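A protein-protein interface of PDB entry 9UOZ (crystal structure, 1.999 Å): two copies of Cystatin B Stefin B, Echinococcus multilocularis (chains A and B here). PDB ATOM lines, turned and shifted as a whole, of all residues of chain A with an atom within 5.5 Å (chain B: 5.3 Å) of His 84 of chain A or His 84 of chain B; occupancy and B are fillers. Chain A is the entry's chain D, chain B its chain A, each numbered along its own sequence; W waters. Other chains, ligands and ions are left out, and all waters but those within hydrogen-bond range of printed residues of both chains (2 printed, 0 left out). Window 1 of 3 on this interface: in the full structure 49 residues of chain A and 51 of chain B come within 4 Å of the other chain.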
ATOM      1  N   TYR A  28     -20.301 -35.667   6.755  1.00  0.00           N
ATOM      2  CA  TYR A  28     -21.514 -34.900   7.013  1.00  0.00           C
ATOM      3  C   TYR A  28     -22.484 -35.008   5.836  1.00  0.00           C
ATOM      4  O   TYR A  28     -23.682 -35.165   6.045  1.00  0.00           O
ATOM      5  CB  TYR A  28     -21.135 -33.447   7.294  1.00  0.00           C
ATOM      6  CG  TYR A  28     -22.324 -32.511   7.421  1.00  0.00           C
ATOM      7  CD1 TYR A  28     -23.017 -32.384   8.613  1.00  0.00           C
ATOM      8  CD2 TYR A  28     -22.733 -31.741   6.343  1.00  0.00           C
ATOM      9  CE1 TYR A  28     -24.108 -31.537   8.727  1.00  0.00           C
ATOM     10  CE2 TYR A  28     -23.820 -30.886   6.440  1.00  0.00           C
ATOM     11  CZ  TYR A  28     -24.507 -30.783   7.631  1.00  0.00           C
ATOM     12  OH  TYR A  28     -25.554 -29.926   7.697  1.00  0.00           O
ATOM     13  N   ASN A  54     -18.604 -21.542  25.097  1.00  0.00           N
ATOM     14  CA  ASN A  54     -19.809 -22.308  24.862  1.00  0.00           C
ATOM     15  C   ASN A  54     -20.504 -22.557  26.202  1.00  0.00           C
ATOM     16  O   ASN A  54     -19.888 -23.037  27.140  1.00  0.00           O
ATOM     17  CB  ASN A  54     -19.537 -23.619  24.150  1.00  0.00           C
ATOM     18  CG  ASN A  54     -19.086 -23.412  22.713  1.00  0.00           C
ATOM     19  OD1 ASN A  54     -19.537 -22.501  22.007  1.00  0.00           O
ATOM     20  ND2 ASN A  54     -18.196 -24.250  22.217  1.00  0.00           N
ATOM     21  N   ARG A  69     -26.876 -25.554  23.215  1.00  0.00           N
ATOM     22  CA  ARG A  69     -25.503 -25.088  23.102  1.00  0.00           C
ATOM     23  C   ARG A  69     -25.514 -23.636  22.633  1.00  0.00           C
ATOM     24  O   ARG A  69     -25.930 -23.341  21.517  1.00  0.00           O
ATOM     25  CB  ARG A  69     -24.788 -25.952  22.062  1.00  0.00           C
ATOM     26  CG  ARG A  69     -23.289 -25.696  22.073  1.00  0.00           C
ATOM     27  CD  ARG A  69     -22.538 -25.749  20.765  1.00  0.00           C
ATOM     28  NE  ARG A  69     -21.922 -27.041  20.510  1.00  0.00           N
ATOM     29  CZ  ARG A  69     -20.683 -27.416  20.159  1.00  0.00           C
ATOM     30  NH1 ARG A  69     -19.630 -26.646  19.945  1.00  0.00           N
ATOM     31  NH2 ARG A  69     -20.552 -28.714  20.012  1.00  0.00           N
ATOM     32  N   VAL A  70     -25.126 -22.704  23.513  1.00  0.00           N
ATOM     33  CA  VAL A  70     -25.112 -21.285  23.202  1.00  0.00           C
ATOM     34  C   VAL A  70     -23.664 -20.789  23.177  1.00  0.00           C
ATOM     35  O   VAL A  70     -22.920 -21.036  24.111  1.00  0.00           O
ATOM     36  CB  VAL A  70     -25.928 -20.529  24.261  1.00  0.00           C
ATOM     37  CG1 VAL A  70     -25.889 -19.026  24.051  1.00  0.00           C
ATOM     38  CG2 VAL A  70     -27.366 -21.022  24.359  1.00  0.00           C
ATOM     39  N   HIS A  71     -23.259 -20.126  22.088  1.00  0.00           N
ATOM     40  CA  HIS A  71     -21.930 -19.549  21.983  1.00  0.00           C
ATOM     41  C   HIS A  71     -21.982 -18.072  22.360  1.00  0.00           C
ATOM     42  O   HIS A  71     -22.817 -17.337  21.855  1.00  0.00           O
ATOM     43  CB  HIS A  71     -21.339 -19.703  20.585  1.00  0.00           C
ATOM     44  CG  HIS A  71     -19.977 -19.104  20.507  1.00  0.00           C
ATOM     45  ND1 HIS A  71     -18.884 -19.679  21.121  1.00  0.00           N
ATOM     46  CD2 HIS A  71     -19.532 -17.959  19.958  1.00  0.00           C
ATOM     47  CE1 HIS A  71     -17.818 -18.918  20.925  1.00  0.00           C
ATOM     48  NE2 HIS A  71     -18.185 -17.863  20.235  1.00  0.00           N
ATOM     49  N   GLU A  82     -25.374 -16.559  20.607  1.00  0.00           N
ATOM     50  CA  GLU A  82     -26.192 -17.260  19.632  1.00  0.00           C
ATOM     51  C   GLU A  82     -26.308 -18.743  19.993  1.00  0.00           C
ATOM     52  O   GLU A  82     -25.372 -19.344  20.507  1.00  0.00           O
ATOM     53  CB  GLU A  82     -25.688 -17.157  18.195  1.00  0.00           C
ATOM     54  CG  GLU A  82     -24.176 -17.113  18.008  1.00  0.00           C
ATOM     55  CD  GLU A  82     -23.668 -16.931  16.596  1.00  0.00           C
ATOM     56  OE1 GLU A  82     -22.519 -17.388  16.385  1.00  0.00           O
ATOM     57  OE2 GLU A  82     -24.357 -16.340  15.726  1.00  0.00           O
ATOM     58  N   VAL A  83     -27.469 -19.333  19.701  1.00  0.00           N
ATOM     59  CA  VAL A  83     -27.658 -20.763  19.849  1.00  0.00           C
ATOM     60  C   VAL A  83     -27.040 -21.466  18.658  1.00  0.00           C
ATOM     61  O   VAL A  83     -27.276 -21.072  17.517  1.00  0.00           O
ATOM     62  CB  VAL A  83     -29.158 -21.108  19.962  1.00  0.00           C
ATOM     63  CG1 VAL A  83     -29.383 -22.608  20.018  1.00  0.00           C
ATOM     64  CG2 VAL A  83     -29.832 -20.430  21.139  1.00  0.00           C
ATOM     65  N   HIS A  84     -26.247 -22.498  18.902  1.00  0.00           N
ATOM     66  CA  HIS A  84     -25.650 -23.259  17.813  1.00  0.00           C
ATOM     67  C   HIS A  84     -26.354 -24.598  17.608  1.00  0.00           C
ATOM     68  O   HIS A  84     -26.332 -25.107  16.495  1.00  0.00           O
ATOM     69  CB  HIS A  84     -24.156 -23.499  18.040  1.00  0.00           C
ATOM     70  CG  HIS A  84     -23.309 -22.288  17.801  1.00  0.00           C
ATOM     71  ND1 HIS A  84     -23.797 -21.053  17.444  1.00  0.00           N
ATOM     72  CD2 HIS A  84     -21.979 -22.150  17.854  1.00  0.00           C
ATOM     73  CE1 HIS A  84     -22.787 -20.228  17.273  1.00  0.00           C
ATOM     74  NE2 HIS A  84     -21.676 -20.867  17.541  1.00  0.00           N
ATOM     75  N   SER A  85     -26.917 -25.201  18.671  1.00  0.00           N
ATOM     76  CA  SER A  85     -27.725 -26.395  18.482  1.00  0.00           C
ATOM     77  C   SER A  85     -28.490 -26.741  19.743  1.00  0.00           C
ATOM     78  O   SER A  85     -28.321 -26.113  20.793  1.00  0.00           O
ATOM     79  CB  SER A  85     -26.944 -27.574  17.964  1.00  0.00           C
ATOM     80  OG  SER A  85     -25.981 -28.068  18.871  1.00  0.00           O
ATOM     81  N   HIS A  86     -29.397 -27.693  19.586  1.00  0.00           N
ATOM     82  CA  HIS A  86     -30.154 -28.243  20.694  1.00  0.00           C
ATOM     83  C   HIS A  86     -30.400 -29.715  20.407  1.00  0.00           C
ATOM     84  O   HIS A  86     -30.296 -30.165  19.273  1.00  0.00           O
ATOM     85  CB  HIS A  86     -31.465 -27.491  20.896  1.00  0.00           C
ATOM     86  CG  HIS A  86     -32.572 -27.950  20.026  1.00  0.00           C
ATOM     87  ND1 HIS A  86     -32.854 -27.449  18.781  1.00  0.00           N
ATOM     88  CD2 HIS A  86     -33.524 -28.863  20.284  1.00  0.00           C
ATOM     89  CE1 HIS A  86     -33.929 -28.068  18.292  1.00  0.00           C
ATOM     90  NE2 HIS A  86     -34.332 -28.951  19.172  1.00  0.00           N
ATOM     91  N   LEU A  99     -23.125 -32.247  20.001  1.00  0.00           N
ATOM     92  CA  LEU A  99     -23.395 -31.545  18.759  1.00  0.00           C
ATOM     93  C   LEU A  99     -24.452 -32.342  18.003  1.00  0.00           C
ATOM     94  O   LEU A  99     -24.202 -33.497  17.709  1.00  0.00           O
ATOM     95  CB  LEU A  99     -22.109 -31.429  17.951  1.00  0.00           C
ATOM     96  CG  LEU A  99     -22.061 -30.319  16.892  1.00  0.00           C
ATOM     97  CD1 LEU A  99     -21.498 -30.916  15.600  1.00  0.00           C
ATOM     98  CD2 LEU A  99     -23.328 -29.473  16.653  1.00  0.00           C
ATOM     99  N   HIS A 101     -27.094 -32.522  14.704  1.00  0.00           N
ATOM    100  CA  HIS A 101     -27.326 -31.937  13.377  1.00  0.00           C
ATOM    101  C   HIS A 101     -28.819 -31.877  13.018  1.00  0.00           C
ATOM    102  O   HIS A 101     -29.479 -32.933  13.150  1.00  0.00           O
ATOM    103  CB  HIS A 101     -26.542 -32.665  12.276  1.00  0.00           C
ATOM    104  CG  HIS A 101     -25.075 -32.466  12.394  1.00  0.00           C
ATOM    105  ND1 HIS A 101     -24.159 -33.472  12.188  1.00  0.00           N
ATOM    106  CD2 HIS A 101     -24.373 -31.385  12.746  1.00  0.00           C
ATOM    107  CE1 HIS A 101     -22.935 -33.003  12.405  1.00  0.00           C
ATOM    108  NE2 HIS A 101     -23.043 -31.737  12.743  1.00  0.00           N
ATOM    109  N   ARG B  69     -20.443 -24.621   7.240  1.00  0.00           N
ATOM    110  CA  ARG B  69     -19.799 -24.003   8.382  1.00  0.00           C
ATOM    111  C   ARG B  69     -19.147 -25.074   9.248  1.00  0.00           C
ATOM    112  O   ARG B  69     -19.863 -25.904   9.812  1.00  0.00           O
ATOM    113  CB  ARG B  69     -20.870 -23.263   9.178  1.00  0.00           C
ATOM    114  CG  ARG B  69     -20.302 -22.436  10.320  1.00  0.00           C
ATOM    115  CD  ARG B  69     -21.412 -21.752  11.051  1.00  0.00           C
ATOM    116  NE  ARG B  69     -20.947 -21.222  12.336  1.00  0.00           N
ATOM    117  CZ  ARG B  69     -21.260 -20.048  12.884  1.00  0.00           C
ATOM    118  NH1 ARG B  69     -20.822 -19.755  14.074  1.00  0.00           N
ATOM    119  NH2 ARG B  69     -21.978 -19.211  12.203  1.00  0.00           N
ATOM    120  N   VAL B  70     -17.795 -25.075   9.298  1.00  0.00           N
ATOM    121  CA  VAL B  70     -17.081 -26.021  10.117  1.00  0.00           C
ATOM    122  C   VAL B  70     -16.361 -25.271  11.238  1.00  0.00           C
ATOM    123  O   VAL B  70     -15.617 -24.337  10.958  1.00  0.00           O
ATOM    124  CB  VAL B  70     -16.099 -26.817   9.236  1.00  0.00           C
ATOM    125  CG1 VAL B  70     -16.763 -27.475   8.042  1.00  0.00           C
ATOM    126  CG2 VAL B  70     -14.967 -25.956   8.784  1.00  0.00           C
ATOM    127  N   HIS B  71     -16.530 -25.717  12.483  1.00  0.00           N
ATOM    128  CA  HIS B  71     -15.770 -25.151  13.596  1.00  0.00           C
ATOM    129  C   HIS B  71     -14.578 -26.044  13.905  1.00  0.00           C
ATOM    130  O   HIS B  71     -14.730 -27.263  14.026  1.00  0.00           O
ATOM    131  CB  HIS B  71     -16.590 -25.027  14.885  1.00  0.00           C
ATOM    132  CG  HIS B  71     -15.726 -24.455  16.030  1.00  0.00           C
ATOM    133  ND1 HIS B  71     -15.265 -25.164  17.119  1.00  0.00           N
ATOM    134  CD2 HIS B  71     -15.202 -23.192  16.191  1.00  0.00           C
ATOM    135  CE1 HIS B  71     -14.525 -24.370  17.895  1.00  0.00           C
ATOM    136  NE2 HIS B  71     -14.465 -23.169  17.345  1.00  0.00           N
ATOM    137  N   GLU B  82     -15.886 -29.935  13.595  1.00  0.00           N
ATOM    138  CA  GLU B  82     -17.277 -30.341  13.486  1.00  0.00           C
ATOM    139  C   GLU B  82     -17.987 -29.401  12.512  1.00  0.00           C
ATOM    140  O   GLU B  82     -17.790 -28.171  12.559  1.00  0.00           O
ATOM    141  CB  GLU B  82     -18.038 -30.186  14.803  1.00  0.00           C
ATOM    142  CG  GLU B  82     -17.323 -30.694  16.057  1.00  0.00           C
ATOM    143  CD  GLU B  82     -17.875 -30.077  17.361  1.00  0.00           C
ATOM    144  OE1 GLU B  82     -18.097 -28.825  17.370  1.00  0.00           O
ATOM    145  OE2 GLU B  82     -18.073 -30.825  18.367  1.00  0.00           O
ATOM    146  N   VAL B  83     -18.863 -29.996  11.702  1.00  0.00           N
ATOM    147  CA  VAL B  83     -19.767 -29.228  10.873  1.00  0.00           C
ATOM    148  C   VAL B  83     -20.916 -28.747  11.752  1.00  0.00           C
ATOM    149  O   VAL B  83     -21.506 -29.535  12.500  1.00  0.00           O
ATOM    150  CB  VAL B  83     -20.318 -30.072   9.709  1.00  0.00           C
ATOM    151  CG1 VAL B  83     -21.377 -29.325   8.913  1.00  0.00           C
ATOM    152  CG2 VAL B  83     -19.218 -30.554   8.791  1.00  0.00           C
ATOM    153  N   HIS B  84     -21.229 -27.452  11.667  1.00  0.00           N
ATOM    154  CA  HIS B  84     -22.367 -26.927  12.388  1.00  0.00           C
ATOM    155  C   HIS B  84     -23.617 -26.827  11.517  1.00  0.00           C
ATOM    156  O   HIS B  84     -24.724 -27.048  11.991  1.00  0.00           O
ATOM    157  CB  HIS B  84     -22.072 -25.578  12.998  1.00  0.00           C
ATOM    158  CG  HIS B  84     -23.385 -24.982  13.321  1.00  0.00           C
ATOM    159  ND1 HIS B  84     -24.183 -24.440  12.342  1.00  0.00           N
ATOM    160  CD2 HIS B  84     -24.114 -24.980  14.451  1.00  0.00           C
ATOM    161  CE1 HIS B  84     -25.345 -24.041  12.882  1.00  0.00           C
ATOM    162  NE2 HIS B  84     -25.314 -24.355  14.173  1.00  0.00           N
ATOM    163  N   SER B  85     -23.428 -26.467  10.242  1.00  0.00           N
ATOM    164  CA  SER B  85     -24.573 -26.361   9.351  1.00  0.00           C
ATOM    165  C   SER B  85     -24.116 -26.154   7.917  1.00  0.00           C
ATOM    166  O   SER B  85     -22.926 -26.024   7.631  1.00  0.00           O
ATOM    167  CB  SER B  85     -25.558 -25.264   9.781  1.00  0.00           C
ATOM    168  OG  SER B  85     -24.988 -23.961   9.726  1.00  0.00           O
ATOM    169  N   HIS B  86     -25.120 -26.204   7.044  1.00  0.00           N
ATOM    170  CA  HIS B  86     -24.923 -25.972   5.633  1.00  0.00           C
ATOM    171  C   HIS B  86     -26.136 -25.241   5.076  1.00  0.00           C
ATOM    172  O   HIS B  86     -27.188 -25.223   5.687  1.00  0.00           O
ATOM    173  CB  HIS B  86     -24.693 -27.307   4.930  1.00  0.00           C
ATOM    174  CG  HIS B  86     -25.954 -28.030   4.577  1.00  0.00           C
ATOM    175  ND1 HIS B  86     -26.561 -27.947   3.339  1.00  0.00           N
ATOM    176  CD2 HIS B  86     -26.664 -28.894   5.270  1.00  0.00           C
ATOM    177  CE1 HIS B  86     -27.695 -28.630   3.368  1.00  0.00           C
ATOM    178  NE2 HIS B  86     -27.662 -29.354   4.449  1.00  0.00           N
ATOM    179  N   LEU B  99     -25.425 -18.715   9.640  1.00  0.00           N
ATOM    180  CA  LEU B  99     -25.782 -19.684  10.646  1.00  0.00           C
ATOM    181  C   LEU B  99     -27.219 -20.074  10.328  1.00  0.00           C
ATOM    182  O   LEU B  99     -28.090 -19.207  10.406  1.00  0.00           O
ATOM    183  CB  LEU B  99     -25.664 -19.042  12.025  1.00  0.00           C
ATOM    184  CG  LEU B  99     -25.580 -20.000  13.227  1.00  0.00           C
ATOM    185  CD1 LEU B  99     -25.706 -19.087  14.408  1.00  0.00           C
ATOM    186  CD2 LEU B  99     -26.591 -21.096  13.384  1.00  0.00           C
ATOM    187  N   GLU B 100     -27.450 -21.360  10.014  1.00  0.00           N
ATOM    188  CA  GLU B 100     -28.780 -21.818   9.613  1.00  0.00           C
ATOM    189  C   GLU B 100     -29.394 -22.730  10.671  1.00  0.00           C
ATOM    190  O   GLU B 100     -28.792 -23.736  11.030  1.00  0.00           O
ATOM    191  CB  GLU B 100     -28.736 -22.633   8.336  1.00  0.00           C
ATOM    192  CG  GLU B 100     -28.531 -21.798   7.084  1.00  0.00           C
ATOM    193  CD  GLU B 100     -29.744 -21.627   6.206  1.00  0.00           C
ATOM    194  OE1 GLU B 100     -30.205 -22.661   5.678  1.00  0.00           O
ATOM    195  OE2 GLU B 100     -30.153 -20.477   5.955  1.00  0.00           O
ATOM    196  N   HIS B 101     -30.564 -22.313  11.177  1.00  0.00           N
ATOM    197  CA  HIS B 101     -31.263 -23.036  12.218  1.00  0.00           C
ATOM    198  C   HIS B 101     -32.341 -23.972  11.680  1.00  0.00           C
ATOM    199  O   HIS B 101     -32.769 -24.858  12.410  1.00  0.00           O
ATOM    200  CB  HIS B 101     -31.844 -22.021  13.211  1.00  0.00           C
ATOM    201  CG  HIS B 101     -30.801 -21.405  14.081  1.00  0.00           C
ATOM    202  ND1 HIS B 101     -29.797 -22.170  14.630  1.00  0.00           N
ATOM    203  CD2 HIS B 101     -30.574 -20.132  14.464  1.00  0.00           C
ATOM    204  CE1 HIS B 101     -29.044 -21.395  15.394  1.00  0.00           C
ATOM    205  NE2 HIS B 101     -29.471 -20.140  15.275  1.00  0.00           N
HETATM  206  O   HOH W   1     -17.675 -23.930  19.109  1.00  0.00           O
HETATM  207  O   HOH W   2     -25.352 -28.037  14.935  1.00  0.00           O
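O of His 84 of chain A is in hydrogen-bond range of NE2 of His 84 of chain B.
NE2 of His 101 of chain A is in hydrogen-bond range of O of Val 83 of chain B.
The side-chain carboxylate (OE1) of Glu 82 of chain B lies within salt-bridge range of the guanidinium group (NH2) of Arg 69 of chain A (3.6 Å).
O of Val 83 of chain A lies close to NE2 of His 101 of chain B (3.3 Å).
NH1 of Arg 69 of chain B is in salt-bridge range of OE1 of Glu 82 of chain A (3.7 Å).
The backbone NH (N) of His 71 of chain A lies within hydrogen-bond range of the backbone carbonyl oxygen (O) of Glu 82 of chain A, at 2.8 Å.
The backbone carbonyl oxygen (O) of Ser 85 of chain B lies within hydrogen-bond range of the backbone NH (N) of Arg 69 of chain B, at 2.9 Å.
The backbone NH (N) of His 84 of chain A is in hydrogen-bond range of the backbone carbonyl oxygen (O) of Arg 69 of chain A (2.8 Å).
O of Arg 69 of chain B lies within hydrogen-bond range of N of His 84 of chain B, at 2.8 Å.
The backbone NH of His 71 of chain B lies within hydrogen-bond range of the backbone carbonyl oxygen of Glu 82 of chain B, 2.8 Å away.
The backbone carbonyl oxygen of Ser 85 of chain A sits at hydrogen-bond distance from the backbone NH of Arg 69 of chain A (2.9 Å).
CD1 of Tyr 28 of chain A touches CG1 of Val 83 of chain B (3.5 Å).
Tyr 28 of chain A touches His 86 of chain B.
CD1 of Leu 99 of chain B touches OE2 of Glu 82 of chain A (3.3 Å).
NE2 of His 84 of chain A touches NH1 of Arg 69 of chain B, at 3.7 Å.
Leu 99 of chain A touches Glu 82 of chain B.
Val 83 of chain B touches Leu 99 of chain A.
Of the printed residues of chain B, His 84 of chain A touches Arg 69 and His 84.
Of chain A, only His 84 (2.6 Å) comes within 4 Å of His 84 of chain B.
Printed residues of chain A within 4 Å of Glu 82 of chain B: Arg 69 and Leu 99.
Of the printed residues of chain B, Arg 69 of chain A touches Glu 82.
Of the printed residues of chain A, His 86 of chain B touches Tyr 28 (2.9 Å).
The nearest printed residue of chain B that does not touch His 84 of chain A is Leu 99 of chain B (4.1 Å).
The nearest printed residue of chain B that does not touch His 101 of chain A is His 84 of chain B (4.4 Å).
Printed residues of chain B that touch a printed residue of chain A: Arg 69, Glu 82, Val 83, His 84, His 86, Leu 99 and His 101.
Hydrophobic or aromatic side chains of chain B that line the printed part of chain A: Val 83, His 84, His 86, Leu 99 and His 101.
Along chain A the printed residues that touch a printed residue of chain B span positions 28 to 101.
Among the printed residues, 11 pairs touch across the chains.
Arg 69 of chain A touches Glu 82 of chain B, and with the chains exchanged Glu 82 of chain A touches Arg 69 of chain B.
His 84 of chain A touches Arg 69 of chain B, but with the chains exchanged Arg 69 of chain A does not touch His 84 of chain B (6.6 Å).
His 84 of chain B touches its own counterpart, His 84 of chain A.
Leu 99 of chain A touches Val 83 of chain B, but with the chains exchanged Val 83 of chain A does not touch Leu 99 of chain B (4.01 Å).
10 positions are printed for both chains.
Water W2 lies within hydrogen-bond range of the backbone carbonyl oxygen of His 84 of chain B and the backbone carbonyl oxygen of His 84 of chain A.
Water W1 lies within hydrogen-bond range of ND2 of Asn 54 of chain A (3.2 Å), ND1 of His 71 of chain B (3.4 Å) and NH1 of Arg 69 of chain A (3.4 Å).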
